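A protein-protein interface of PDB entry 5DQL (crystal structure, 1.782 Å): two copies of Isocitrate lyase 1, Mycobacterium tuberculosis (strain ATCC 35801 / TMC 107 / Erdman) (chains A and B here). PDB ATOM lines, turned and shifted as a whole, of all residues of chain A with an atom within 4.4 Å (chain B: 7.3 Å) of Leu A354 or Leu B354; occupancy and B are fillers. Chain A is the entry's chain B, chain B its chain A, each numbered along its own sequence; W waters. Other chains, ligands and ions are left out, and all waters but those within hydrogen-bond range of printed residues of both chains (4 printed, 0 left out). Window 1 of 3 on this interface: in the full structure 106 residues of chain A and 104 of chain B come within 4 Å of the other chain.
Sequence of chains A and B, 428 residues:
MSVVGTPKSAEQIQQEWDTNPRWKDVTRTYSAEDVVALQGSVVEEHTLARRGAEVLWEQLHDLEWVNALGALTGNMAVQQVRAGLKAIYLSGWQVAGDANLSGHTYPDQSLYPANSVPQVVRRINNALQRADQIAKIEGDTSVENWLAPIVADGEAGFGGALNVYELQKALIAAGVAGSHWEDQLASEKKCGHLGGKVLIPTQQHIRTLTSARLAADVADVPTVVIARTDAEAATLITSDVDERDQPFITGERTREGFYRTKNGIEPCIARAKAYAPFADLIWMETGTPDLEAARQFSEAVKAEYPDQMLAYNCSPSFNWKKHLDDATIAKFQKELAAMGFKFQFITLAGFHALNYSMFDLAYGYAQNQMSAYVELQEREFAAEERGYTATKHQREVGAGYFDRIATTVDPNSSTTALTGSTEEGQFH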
ATOM      1  N   THR A  73     -22.425  18.414  -6.354  1.00  0.00           N
ATOM      2  CA  THR A  73     -22.494  19.082  -5.051  1.00  0.00           C
ATOM      3  C   THR A  73     -23.950  19.140  -4.583  1.00  0.00           C
ATOM      4  O   THR A  73     -24.877  18.921  -5.374  1.00  0.00           O
ATOM      5  CB  THR A  73     -21.927  20.527  -5.073  1.00  0.00           C
ATOM      6  OG1 THR A  73     -22.904  21.415  -5.645  1.00  0.00           O
ATOM      7  CG2 THR A  73     -20.616  20.608  -5.861  1.00  0.00           C
ATOM      8  N   ASN A  75     -25.667  21.842  -3.523  1.00  0.00           N
ATOM      9  CA  ASN A  75     -26.318  22.988  -4.176  1.00  0.00           C
ATOM     10  C   ASN A  75     -26.799  22.662  -5.602  1.00  0.00           C
ATOM     11  O   ASN A  75     -27.840  23.162  -6.034  1.00  0.00           O
ATOM     12  CB  ASN A  75     -25.366  24.179  -4.256  1.00  0.00           C
ATOM     13  CG  ASN A  75     -25.203  24.933  -2.928  1.00  0.00           C
ATOM     14  OD1 ASN A  75     -24.572  25.990  -2.904  1.00  0.00           O
ATOM     15  ND2 ASN A  75     -25.737  24.392  -1.832  1.00  0.00           N
ATOM     16  N   MET A  76     -26.039  21.852  -6.348  1.00  0.00           N
ATOM     17  CA  MET A  76     -26.461  21.463  -7.701  1.00  0.00           C
ATOM     18  C   MET A  76     -27.793  20.722  -7.682  1.00  0.00           C
ATOM     19  O   MET A  76     -28.699  21.011  -8.472  1.00  0.00           O
ATOM     20  CB  MET A  76     -25.422  20.553  -8.383  1.00  0.00           C
ATOM     21  CG  MET A  76     -24.357  21.278  -9.183  1.00  0.00           C
ATOM     22  SD  MET A  76     -23.271  20.113 -10.045  1.00  0.00           S
ATOM     23  CE  MET A  76     -22.014  21.272 -10.595  1.00  0.00           C
ATOM     24  N   ASP A  98     -14.009  15.526  -9.471  1.00  0.00           N
ATOM     25  CA  ASP A  98     -14.086  16.783  -8.708  1.00  0.00           C
ATOM     26  C   ASP A  98     -14.727  16.654  -7.324  1.00  0.00           C
ATOM     27  O   ASP A  98     -14.931  17.660  -6.635  1.00  0.00           O
ATOM     28  CB  ASP A  98     -14.819  17.844  -9.559  1.00  0.00           C
ATOM     29  CG  ASP A  98     -14.479  19.294  -9.164  1.00  0.00           C
ATOM     30  OD1 ASP A  98     -13.397  19.558  -8.591  1.00  0.00           O
ATOM     31  OD2 ASP A  98     -15.317  20.180  -9.442  1.00  0.00           O
ATOM     32  N   GLY A 350     -23.265  18.059 -14.492  1.00  0.00           N
ATOM     33  CA  GLY A 350     -22.629  18.893 -13.488  1.00  0.00           C
ATOM     34  C   GLY A 350     -21.234  19.356 -13.845  1.00  0.00           C
ATOM     35  O   GLY A 350     -20.928  20.549 -13.721  1.00  0.00           O
ATOM     36  N   PHE A 351     -20.382  18.419 -14.267  1.00  0.00           N
ATOM     37  CA  PHE A 351     -19.020  18.766 -14.637  1.00  0.00           C
ATOM     38  C   PHE A 351     -19.007  19.879 -15.698  1.00  0.00           C
ATOM     39  O   PHE A 351     -18.269  20.856 -15.576  1.00  0.00           O
ATOM     40  CB  PHE A 351     -18.241  17.525 -15.090  1.00  0.00           C
ATOM     41  CG  PHE A 351     -16.895  17.835 -15.675  1.00  0.00           C
ATOM     42  CD1 PHE A 351     -16.761  18.114 -17.038  1.00  0.00           C
ATOM     43  CD2 PHE A 351     -15.763  17.848 -14.873  1.00  0.00           C
ATOM     44  CE1 PHE A 351     -15.515  18.417 -17.588  1.00  0.00           C
ATOM     45  CE2 PHE A 351     -14.507  18.133 -15.414  1.00  0.00           C
ATOM     46  CZ  PHE A 351     -14.382  18.419 -16.772  1.00  0.00           C
ATOM     47  N   HIS A 352     -19.835  19.751 -16.726  1.00  0.00           N
ATOM     48  CA  HIS A 352     -19.804  20.747 -17.793  1.00  0.00           C
ATOM     49  C   HIS A 352     -20.381  22.100 -17.402  1.00  0.00           C
ATOM     50  O   HIS A 352     -19.800  23.145 -17.705  1.00  0.00           O
ATOM     51  CB  HIS A 352     -20.455  20.192 -19.043  1.00  0.00           C
ATOM     52  CG  HIS A 352     -19.618  19.154 -19.703  1.00  0.00           C
ATOM     53  ND1 HIS A 352     -18.487  19.471 -20.432  1.00  0.00           N
ATOM     54  CD2 HIS A 352     -19.694  17.802 -19.695  1.00  0.00           C
ATOM     55  CE1 HIS A 352     -17.929  18.359 -20.874  1.00  0.00           C
ATOM     56  NE2 HIS A 352     -18.638  17.331 -20.435  1.00  0.00           N
ATOM     57  N   ALA A 353     -21.514  22.078 -16.721  1.00  0.00           N
ATOM     58  CA  ALA A 353     -22.139  23.325 -16.263  1.00  0.00           C
ATOM     59  C   ALA A 353     -21.211  24.097 -15.340  1.00  0.00           C
ATOM     60  O   ALA A 353     -21.058  25.325 -15.467  1.00  0.00           O
ATOM     61  CB  ALA A 353     -23.454  23.030 -15.586  1.00  0.00           C
ATOM     62  N   LEU A 354     -20.580  23.379 -14.412  1.00  0.00           N
ATOM     63  CA  LEU A 354     -19.640  23.989 -13.478  1.00  0.00           C
ATOM     64  C   LEU A 354     -18.396  24.518 -14.180  1.00  0.00           C
ATOM     65  O   LEU A 354     -17.965  25.654 -13.939  1.00  0.00           O
ATOM     66  CB  LEU A 354     -19.232  22.980 -12.384  1.00  0.00           C
ATOM     67  CG  LEU A 354     -18.269  23.485 -11.309  1.00  0.00           C
ATOM     68  CD1 LEU A 354     -18.514  22.727 -10.016  1.00  0.00           C
ATOM     69  CD2 LEU A 354     -16.820  23.307 -11.736  1.00  0.00           C
ATOM     70  N   ASN A 355     -17.777  23.681 -15.006  1.00  0.00           N
ATOM     71  CA  ASN A 355     -16.534  24.083 -15.654  1.00  0.00           C
ATOM     72  C   ASN A 355     -16.761  25.211 -16.652  1.00  0.00           C
ATOM     73  O   ASN A 355     -15.977  26.168 -16.699  1.00  0.00           O
ATOM     74  CB  ASN A 355     -15.844  22.899 -16.341  1.00  0.00           C
ATOM     75  CG  ASN A 355     -15.084  22.021 -15.358  1.00  0.00           C
ATOM     76  OD1 ASN A 355     -13.878  22.190 -15.163  1.00  0.00           O
ATOM     77  ND2 ASN A 355     -15.788  21.087 -14.723  1.00  0.00           N
ATOM     78  N   TYR A 356     -17.819  25.103 -17.455  1.00  0.00           N
ATOM     79  CA  TYR A 356     -18.045  26.137 -18.471  1.00  0.00           C
ATOM     80  C   TYR A 356     -18.428  27.458 -17.819  1.00  0.00           C
ATOM     81  O   TYR A 356     -17.951  28.525 -18.220  1.00  0.00           O
ATOM     82  CB  TYR A 356     -19.104  25.755 -19.508  1.00  0.00           C
ATOM     83  CG  TYR A 356     -19.342  26.915 -20.468  1.00  0.00           C
ATOM     84  CD1 TYR A 356     -18.367  27.275 -21.390  1.00  0.00           C
ATOM     85  CD2 TYR A 356     -20.508  27.679 -20.405  1.00  0.00           C
ATOM     86  CE1 TYR A 356     -18.547  28.349 -22.242  1.00  0.00           C
ATOM     87  CE2 TYR A 356     -20.701  28.759 -21.254  1.00  0.00           C
ATOM     88  CZ  TYR A 356     -19.717  29.087 -22.174  1.00  0.00           C
ATOM     89  OH  TYR A 356     -19.891  30.152 -23.030  1.00  0.00           O
ATOM     90  N   SER A 357     -19.288  27.408 -16.808  1.00  0.00           N
ATOM     91  CA  SER A 357     -19.712  28.664 -16.194  1.00  0.00           C
ATOM     92  C   SER A 357     -18.563  29.393 -15.503  1.00  0.00           C
ATOM     93  O   SER A 357     -18.533  30.627 -15.489  1.00  0.00           O
ATOM     94  CB  SER A 357     -20.877  28.457 -15.234  1.00  0.00           C
ATOM     95  OG  SER A 357     -20.468  27.667 -14.126  1.00  0.00           O
ATOM     96  N   MET A 358     -17.605  28.656 -14.941  1.00  0.00           N
ATOM     97  CA  MET A 358     -16.501  29.326 -14.265  1.00  0.00           C
ATOM     98  C   MET A 358     -15.453  29.804 -15.248  1.00  0.00           C
ATOM     99  O   MET A 358     -14.792  30.827 -15.010  1.00  0.00           O
ATOM    100  CB  MET A 358     -15.834  28.440 -13.213  1.00  0.00           C
ATOM    101  CG  MET A 358     -14.751  29.179 -12.400  1.00  0.00           C
ATOM    102  SD  MET A 358     -15.275  30.767 -11.663  1.00  0.00           S
ATOM    103  CE  MET A 358     -16.451  30.172 -10.442  1.00  0.00           C
ATOM    104  N   LEU B  72     -14.829  26.978  -4.944  1.00  0.00           N
ATOM    105  CA  LEU B  72     -15.208  25.990  -3.934  1.00  0.00           C
ATOM    106  C   LEU B  72     -14.944  24.540  -4.349  1.00  0.00           C
ATOM    107  O   LEU B  72     -15.092  23.633  -3.526  1.00  0.00           O
ATOM    108  CB  LEU B  72     -16.659  26.175  -3.491  1.00  0.00           C
ATOM    109  CG  LEU B  72     -17.746  25.895  -4.521  1.00  0.00           C
ATOM    110  CD1 LEU B  72     -18.517  24.649  -4.120  1.00  0.00           C
ATOM    111  CD2 LEU B  72     -18.687  27.096  -4.604  1.00  0.00           C
ATOM    112  N   THR B  73     -14.583  24.322  -5.617  1.00  0.00           N
ATOM    113  CA  THR B  73     -14.066  23.027  -6.061  1.00  0.00           C
ATOM    114  C   THR B  73     -12.734  23.158  -6.780  1.00  0.00           C
ATOM    115  O   THR B  73     -12.337  24.254  -7.216  1.00  0.00           O
ATOM    116  CB  THR B  73     -15.028  22.259  -7.016  1.00  0.00           C
ATOM    117  OG1 THR B  73     -14.885  22.765  -8.345  1.00  0.00           O
ATOM    118  CG2 THR B  73     -16.472  22.367  -6.579  1.00  0.00           C
ATOM    119  N   GLY B  74     -12.044  22.028  -6.905  1.00  0.00           N
ATOM    120  CA  GLY B  74     -10.786  21.988  -7.631  1.00  0.00           C
ATOM    121  C   GLY B  74     -10.931  22.407  -9.090  1.00  0.00           C
ATOM    122  O   GLY B  74     -10.160  23.249  -9.580  1.00  0.00           O
ATOM    123  N   ASN B  75     -11.916  21.842  -9.781  1.00  0.00           N
ATOM    124  CA  ASN B  75     -12.155  22.192 -11.189  1.00  0.00           C
ATOM    125  C   ASN B  75     -12.427  23.696 -11.339  1.00  0.00           C
ATOM    126  O   ASN B  75     -12.105  24.301 -12.373  1.00  0.00           O
ATOM    127  CB  ASN B  75     -13.345  21.409 -11.765  1.00  0.00           C
ATOM    128  CG  ASN B  75     -13.037  19.928 -12.045  1.00  0.00           C
ATOM    129  OD1 ASN B  75     -13.843  19.250 -12.678  1.00  0.00           O
ATOM    130  ND2 ASN B  75     -11.915  19.420 -11.547  1.00  0.00           N
ATOM    131  N   MET B  76     -13.027  24.302 -10.316  1.00  0.00           N
ATOM    132  CA  MET B  76     -13.351  25.732 -10.393  1.00  0.00           C
ATOM    133  C   MET B  76     -12.070  26.542 -10.460  1.00  0.00           C
ATOM    134  O   MET B  76     -11.980  27.529 -11.208  1.00  0.00           O
ATOM    135  CB  MET B  76     -14.157  26.199  -9.178  1.00  0.00           C
ATOM    136  CG  MET B  76     -15.644  26.125  -9.325  1.00  0.00           C
ATOM    137  SD  MET B  76     -16.432  27.132  -8.030  1.00  0.00           S
ATOM    138  CE  MET B  76     -18.096  26.509  -8.214  1.00  0.00           C
ATOM    139  N   ALA B  77     -11.083  26.128  -9.669  1.00  0.00           N
ATOM    140  CA  ALA B  77      -9.797  26.812  -9.635  1.00  0.00           C
ATOM    141  C   ALA B  77      -9.048  26.596 -10.943  1.00  0.00           C
ATOM    142  O   ALA B  77      -8.388  27.507 -11.447  1.00  0.00           O
ATOM    143  CB  ALA B  77      -8.963  26.329  -8.463  1.00  0.00           C
ATOM    144  N   GLN B  79     -10.315  26.198 -13.941  1.00  0.00           N
ATOM    145  CA  GLN B  79     -10.882  27.081 -14.962  1.00  0.00           C
ATOM    146  C   GLN B  79     -10.435  28.533 -14.745  1.00  0.00           C
ATOM    147  O   GLN B  79     -10.100  29.230 -15.702  1.00  0.00           O
ATOM    148  CB  GLN B  79     -12.417  27.001 -15.006  1.00  0.00           C
ATOM    149  CG  GLN B  79     -12.997  25.653 -15.488  1.00  0.00           C
ATOM    150  CD  GLN B  79     -12.343  25.135 -16.764  1.00  0.00           C
ATOM    151  OE1 GLN B  79     -12.065  25.897 -17.690  1.00  0.00           O
ATOM    152  NE2 GLN B  79     -12.088  23.836 -16.811  1.00  0.00           N
ATOM    153  N   ASP B  98     -21.591  24.769   0.830  1.00  0.00           N
ATOM    154  CA  ASP B  98     -21.577  23.681  -0.162  1.00  0.00           C
ATOM    155  C   ASP B  98     -20.297  22.828  -0.197  1.00  0.00           C
ATOM    156  O   ASP B  98     -20.144  22.009  -1.092  1.00  0.00           O
ATOM    157  CB  ASP B  98     -21.826  24.296  -1.553  1.00  0.00           C
ATOM    158  CG  ASP B  98     -22.438  23.311  -2.566  1.00  0.00           C
ATOM    159  OD1 ASP B  98     -23.087  22.305  -2.170  1.00  0.00           O
ATOM    160  OD2 ASP B  98     -22.279  23.571  -3.794  1.00  0.00           O
ATOM    161  N   LEU B 348     -18.053  35.223  -3.258  1.00  0.00           N
ATOM    162  CA  LEU B 348     -19.061  34.209  -3.579  1.00  0.00           C
ATOM    163  C   LEU B 348     -19.241  33.927  -5.073  1.00  0.00           C
ATOM    164  O   LEU B 348     -20.301  33.459  -5.485  1.00  0.00           O
ATOM    165  CB  LEU B 348     -20.422  34.597  -2.993  1.00  0.00           C
ATOM    166  CG  LEU B 348     -20.419  34.949  -1.513  1.00  0.00           C
ATOM    167  CD1 LEU B 348     -21.852  34.968  -0.987  1.00  0.00           C
ATOM    168  CD2 LEU B 348     -19.576  33.955  -0.739  1.00  0.00           C
ATOM    169  N   ALA B 349     -18.210  34.199  -5.871  1.00  0.00           N
ATOM    170  CA  ALA B 349     -18.272  33.998  -7.327  1.00  0.00           C
ATOM    171  C   ALA B 349     -18.622  32.556  -7.684  1.00  0.00           C
ATOM    172  O   ALA B 349     -19.458  32.291  -8.563  1.00  0.00           O
ATOM    173  CB  ALA B 349     -16.940  34.408  -7.992  1.00  0.00           C
ATOM    174  N   GLY B 350     -17.988  31.613  -6.999  1.00  0.00           N
ATOM    175  CA  GLY B 350     -18.241  30.214  -7.302  1.00  0.00           C
ATOM    176  C   GLY B 350     -19.641  29.756  -6.934  1.00  0.00           C
ATOM    177  O   GLY B 350     -20.261  29.013  -7.686  1.00  0.00           O
ATOM    178  N   PHE B 351     -20.136  30.171  -5.768  1.00  0.00           N
ATOM    179  CA  PHE B 351     -21.506  29.852  -5.387  1.00  0.00           C
ATOM    180  C   PHE B 351     -22.494  30.276  -6.471  1.00  0.00           C
ATOM    181  O   PHE B 351     -23.404  29.526  -6.851  1.00  0.00           O
ATOM    182  CB  PHE B 351     -21.884  30.546  -4.078  1.00  0.00           C
ATOM    183  CG  PHE B 351     -23.332  30.356  -3.696  1.00  0.00           C
ATOM    184  CD1 PHE B 351     -23.734  29.220  -3.002  1.00  0.00           C
ATOM    185  CD2 PHE B 351     -24.295  31.300  -4.045  1.00  0.00           C
ATOM    186  CE1 PHE B 351     -25.061  29.032  -2.644  1.00  0.00           C
ATOM    187  CE2 PHE B 351     -25.633  31.118  -3.697  1.00  0.00           C
ATOM    188  CZ  PHE B 351     -26.020  29.985  -2.995  1.00  0.00           C
ATOM    189  N   HIS B 352     -22.339  31.507  -6.948  1.00  0.00           N
ATOM    190  CA  HIS B 352     -23.319  32.044  -7.873  1.00  0.00           C
ATOM    191  C   HIS B 352     -23.220  31.423  -9.253  1.00  0.00           C
ATOM    192  O   HIS B 352     -24.232  31.023  -9.823  1.00  0.00           O
ATOM    193  CB  HIS B 352     -23.275  33.579  -7.898  1.00  0.00           C
ATOM    194  CG  HIS B 352     -23.893  34.192  -6.678  1.00  0.00           C
ATOM    195  ND1 HIS B 352     -25.251  34.178  -6.454  1.00  0.00           N
ATOM    196  CD2 HIS B 352     -23.332  34.777  -5.592  1.00  0.00           C
ATOM    197  CE1 HIS B 352     -25.506  34.749  -5.282  1.00  0.00           C
ATOM    198  NE2 HIS B 352     -24.361  35.122  -4.745  1.00  0.00           N
ATOM    199  N   ALA B 353     -22.004  31.314  -9.770  1.00  0.00           N
ATOM    200  CA  ALA B 353     -21.816  30.675 -11.065  1.00  0.00           C
ATOM    201  C   ALA B 353     -22.356  29.249 -11.056  1.00  0.00           C
ATOM    202  O   ALA B 353     -22.985  28.815 -12.020  1.00  0.00           O
ATOM    203  CB  ALA B 353     -20.348  30.692 -11.468  1.00  0.00           C
ATOM    204  N   LEU B 354     -22.100  28.503  -9.982  1.00  0.00           N
ATOM    205  CA  LEU B 354     -22.553  27.109  -9.924  1.00  0.00           C
ATOM    206  C   LEU B 354     -24.066  27.019  -9.829  1.00  0.00           C
ATOM    207  O   LEU B 354     -24.701  26.222 -10.537  1.00  0.00           O
ATOM    208  CB  LEU B 354     -21.913  26.366  -8.736  1.00  0.00           C
ATOM    209  CG  LEU B 354     -22.338  24.913  -8.432  1.00  0.00           C
ATOM    210  CD1 LEU B 354     -21.229  24.190  -7.686  1.00  0.00           C
ATOM    211  CD2 LEU B 354     -23.621  24.842  -7.600  1.00  0.00           C
ATOM    212  N   ASN B 355     -24.640  27.784  -8.904  1.00  0.00           N
ATOM    213  CA  ASN B 355     -26.080  27.709  -8.678  1.00  0.00           C
ATOM    214  C   ASN B 355     -26.847  28.209  -9.902  1.00  0.00           C
ATOM    215  O   ASN B 355     -27.817  27.587 -10.326  1.00  0.00           O
ATOM    216  CB  ASN B 355     -26.495  28.474  -7.404  1.00  0.00           C
ATOM    217  CG  ASN B 355     -26.280  27.651  -6.133  1.00  0.00           C
ATOM    218  OD1 ASN B 355     -27.196  26.971  -5.652  1.00  0.00           O
ATOM    219  ND2 ASN B 355     -25.067  27.713  -5.585  1.00  0.00           N
ATOM    220  N   TYR B 356     -26.388  29.308 -10.492  1.00  0.00           N
ATOM    221  CA  TYR B 356     -27.087  29.848 -11.658  1.00  0.00           C
ATOM    222  C   TYR B 356     -26.934  28.915 -12.858  1.00  0.00           C
ATOM    223  O   TYR B 356     -27.914  28.610 -13.551  1.00  0.00           O
ATOM    224  CB  TYR B 356     -26.611  31.261 -12.025  1.00  0.00           C
ATOM    225  CG  TYR B 356     -27.327  31.764 -13.274  1.00  0.00           C
ATOM    226  CD1 TYR B 356     -28.686  32.034 -13.243  1.00  0.00           C
ATOM    227  CD2 TYR B 356     -26.654  31.907 -14.486  1.00  0.00           C
ATOM    228  CE1 TYR B 356     -29.366  32.459 -14.380  1.00  0.00           C
ATOM    229  CE2 TYR B 356     -27.323  32.328 -15.628  1.00  0.00           C
ATOM    230  CZ  TYR B 356     -28.679  32.599 -15.564  1.00  0.00           C
ATOM    231  OH  TYR B 356     -29.353  33.020 -16.684  1.00  0.00           O
ATOM    232  N   SER B 357     -25.717  28.448 -13.110  1.00  0.00           N
ATOM    233  CA  SER B 357     -25.516  27.626 -14.309  1.00  0.00           C
ATOM    234  C   SER B 357     -26.295  26.328 -14.219  1.00  0.00           C
ATOM    235  O   SER B 357     -26.895  25.895 -15.198  1.00  0.00           O
ATOM    236  CB  SER B 357     -24.037  27.359 -14.586  1.00  0.00           C
ATOM    237  OG  SER B 357     -23.466  26.517 -13.607  1.00  0.00           O
ATOM    238  N   MET B 358     -26.316  25.698 -13.047  1.00  0.00           N
ATOM    239  CA  MET B 358     -27.140  24.505 -12.917  1.00  0.00           C
ATOM    240  C   MET B 358     -28.642  24.813 -12.945  1.00  0.00           C
ATOM    241  O   MET B 358     -29.418  24.023 -13.478  1.00  0.00           O
ATOM    242  CB  MET B 358     -26.781  23.679 -11.667  1.00  0.00           C
ATOM    243  CG  MET B 358     -27.569  22.358 -11.575  1.00  0.00           C
ATOM    244  SD  MET B 358     -27.470  21.308 -13.072  1.00  0.00           S
ATOM    245  CE  MET B 358     -25.714  20.939 -13.034  1.00  0.00           C
ATOM    246  N   PHE B 359     -29.077  25.934 -12.367  1.00  0.00           N
ATOM    247  CA  PHE B 359     -30.507  26.247 -12.453  1.00  0.00           C
ATOM    248  C   PHE B 359     -30.947  26.423 -13.914  1.00  0.00           C
ATOM    249  O   PHE B 359     -31.978  25.896 -14.338  1.00  0.00           O
ATOM    250  CB  PHE B 359     -30.907  27.495 -11.649  1.00  0.00           C
ATOM    251  CG  PHE B 359     -32.331  27.922 -11.910  1.00  0.00           C
ATOM    252  CD1 PHE B 359     -33.370  27.397 -11.150  1.00  0.00           C
ATOM    253  CD2 PHE B 359     -32.637  28.819 -12.948  1.00  0.00           C
ATOM    254  CE1 PHE B 359     -34.697  27.755 -11.402  1.00  0.00           C
ATOM    255  CE2 PHE B 359     -33.959  29.185 -13.211  1.00  0.00           C
ATOM    256  CZ  PHE B 359     -34.993  28.654 -12.435  1.00  0.00           C
ATOM    257  N   ASP B 360     -30.155  27.176 -14.661  1.00  0.00           N
ATOM    258  CA  ASP B 360     -30.457  27.522 -16.055  1.00  0.00           C
ATOM    259  C   ASP B 360     -30.525  26.236 -16.888  1.00  0.00           C
ATOM    260  O   ASP B 360     -31.513  25.991 -17.591  1.00  0.00           O
ATOM    261  CB  ASP B 360     -29.373  28.486 -16.551  1.00  0.00           C
ATOM    262  CG  ASP B 360     -29.607  28.974 -17.962  1.00  0.00           C
ATOM    263  OD1 ASP B 360     -30.748  29.387 -18.279  1.00  0.00           O
ATOM    264  OD2 ASP B 360     -28.628  28.962 -18.744  1.00  0.00           O
ATOM    265  N   LEU B 361     -29.502  25.384 -16.767  1.00  0.00           N
ATOM    266  CA  LEU B 361     -29.496  24.098 -17.478  1.00  0.00           C
ATOM    267  C   LEU B 361     -30.659  23.196 -17.062  1.00  0.00           C
ATOM    268  O   LEU B 361     -31.340  22.609 -17.914  1.00  0.00           O
ATOM    269  CB  LEU B 361     -28.152  23.357 -17.304  1.00  0.00           C
ATOM    270  CG  LEU B 361     -28.046  21.979 -17.974  1.00  0.00           C
ATOM    271  CD1 LEU B 361     -28.092  22.098 -19.495  1.00  0.00           C
ATOM    272  CD2 LEU B 361     -26.779  21.236 -17.529  1.00  0.00           C
ATOM    273  N   LEU B 376     -25.562  24.106 -24.212  1.00  0.00           N
ATOM    274  CA  LEU B 376     -24.362  24.211 -23.377  1.00  0.00           C
ATOM    275  C   LEU B 376     -23.132  23.648 -24.091  1.00  0.00           C
ATOM    276  O   LEU B 376     -22.098  24.327 -24.175  1.00  0.00           O
ATOM    277  CB  LEU B 376     -24.565  23.509 -22.028  1.00  0.00           C
ATOM    278  CG  LEU B 376     -23.340  23.465 -21.107  1.00  0.00           C
ATOM    279  CD1 LEU B 376     -22.825  24.873 -20.821  1.00  0.00           C
ATOM    280  CD2 LEU B 376     -23.695  22.742 -19.809  1.00  0.00           C
ATOM    281  N   TYR B 388     -10.819  27.388 -23.669  1.00  0.00           N
ATOM    282  CA  TYR B 388     -11.561  26.376 -22.922  1.00  0.00           C
ATOM    283  C   TYR B 388     -11.217  24.991 -23.448  1.00  0.00           C
ATOM    284  O   TYR B 388     -11.171  24.772 -24.667  1.00  0.00           O
ATOM    285  CB  TYR B 388     -13.056  26.623 -23.073  1.00  0.00           C
ATOM    286  CG  TYR B 388     -13.963  25.736 -22.229  1.00  0.00           C
ATOM    287  CD1 TYR B 388     -14.048  25.902 -20.852  1.00  0.00           C
ATOM    288  CD2 TYR B 388     -14.756  24.754 -22.821  1.00  0.00           C
ATOM    289  CE1 TYR B 388     -14.899  25.119 -20.090  1.00  0.00           C
ATOM    290  CE2 TYR B 388     -15.607  23.957 -22.056  1.00  0.00           C
ATOM    291  CZ  TYR B 388     -15.670  24.146 -20.696  1.00  0.00           C
ATOM    292  OH  TYR B 388     -16.514  23.373 -19.927  1.00  0.00           O
HETATM  293  O   HOH W   1     -13.409  19.656  -5.491  1.00  0.00           O
HETATM  294  O   HOH W   2     -16.649  19.386 -11.750  1.00  0.00           O
HETATM  295  O   HOH W   3     -22.018  26.303  -4.009  1.00  0.00           O
HETATM  296  O   HOH W   4     -11.155  21.113 -14.854  1.00  0.00           O
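Leu A354 touches four residues of chain B. Of the printed residues of chain A, Leu B376 touches Ala A353 and Tyr A356. Printed residues of chain A within 4 Å of Asp B98: Thr A73 and Asn A75. The nearest residue of chain B that does not touch Leu A354 is Ser B357 (4.3 Å). The nearest printed residue of chain A that does not touch Leu B354 is Ser A357 (4.5 Å).
SD of Met B76 is in hydrogen-bond range of N of Leu B72, 3.5 Å away. N of Asn B75 sits close to OG1 of Thr B73 (3.4 Å). OG1 of Thr B73 lies within hydrogen-bond range of N of Met B76 (3.1 Å).
OD2 of Asp A98 is in hydrogen-bond range of OG1 of Thr B73, 2.8 Å away. The backbone NH (N) of Gly B74 sits at hydrogen-bond distance from the side-chain carboxylate (OD1) of Asp A98, 3.3 Å away. OD1 of Asp A98 is in hydrogen-bond range of N of Asn B75 (3.0 Å). OD1 of Asn B75 lies within hydrogen-bond range of ND2 of Asn A355. The side-chain amide nitrogen of Gln B79 lies within hydrogen-bond range of the side-chain amide oxygen of Asn A355 (2.9 Å). OD2 of Asp B98 sits at hydrogen-bond distance from OG1 of Thr A73. N of Asn A75 lies within hydrogen-bond range of OD1 of Asp B98 (2.9 Å). The backbone carbonyl oxygen (O) of Ala B353 lies within hydrogen-bond range of the side-chain hydroxyl (OG) of Ser A357 (3.5 Å). The side-chain amide oxygen (OD1) of Asn A75 lies within hydrogen-bond range of the side-chain amide nitrogen (ND2) of Asn B355 (3.2 Å). O of Ala A353 sits at hydrogen-bond distance from OG of Ser B357, at 3.3 Å. The side-chain hydroxyl of Ser A357 lies within hydrogen-bond range of the side-chain hydroxyl of Ser B357, at 3.3 Å. The backbone NH (N) of Tyr A356 lies within hydrogen-bond range of the side-chain hydroxyl (OH) of Tyr B388 (3.3 Å).
Thr A73 touches Asp B98, and with the chains exchanged Asp A98 touches Thr B73. Thr A73 touches Leu B354, and with the chains exchanged Leu A354 touches Thr B73. Ala A353 touches Ser B357, and with the chains exchanged Ser A357 touches Ala B353. Leu B354 touches its own counterpart, Leu A354.
CD2 of Leu B354 touches CB of Asn A75, at 3.8 Å. Asn B75 touches Phe A351 (OD1 to CE2, 3.0 Å). His A352 touches Tyr B388. Met B358 touches Ala A353. Leu B376 touches Ala A353 (CD2 to N, 3.8 Å). Met B76 touches Leu A354. OH of Tyr B388 touches CB of Asn A355, at 3.7 Å. Met A358 touches Gly B350 (CE to CA, 3.6 Å).
Hydrophobic or aromatic side chains of chain A within 4 Å of the printed part of chain B: Met A76, Phe A351, Ala A353, Leu A354, Tyr A356 and Met A358. Hydrophobic or aromatic side chains of chain B within 4 Å of the printed part of chain A: Met B76, Phe B351, Leu B354, Met B358, Leu B376 and Tyr B388. Among the printed residues, 30 pairs touch across the chains. Among the printed residues, no Asp or Glu carboxylate lies within 4 Å of a Lys or Arg side-chain nitrogen of the other chain.
Water W3 bridges OD2 of Asp B98 (2.8 Å) and OD1 of Asn A75 (2.8 Å). Water W1 lies within hydrogen-bond range of O of Asp A98 (2.8 Å) and N of Gly B74 (3.1 Å). Water W4 bridges the side-chain amide oxygen of Asn A355 and the side-chain amide nitrogen of Gln B79.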
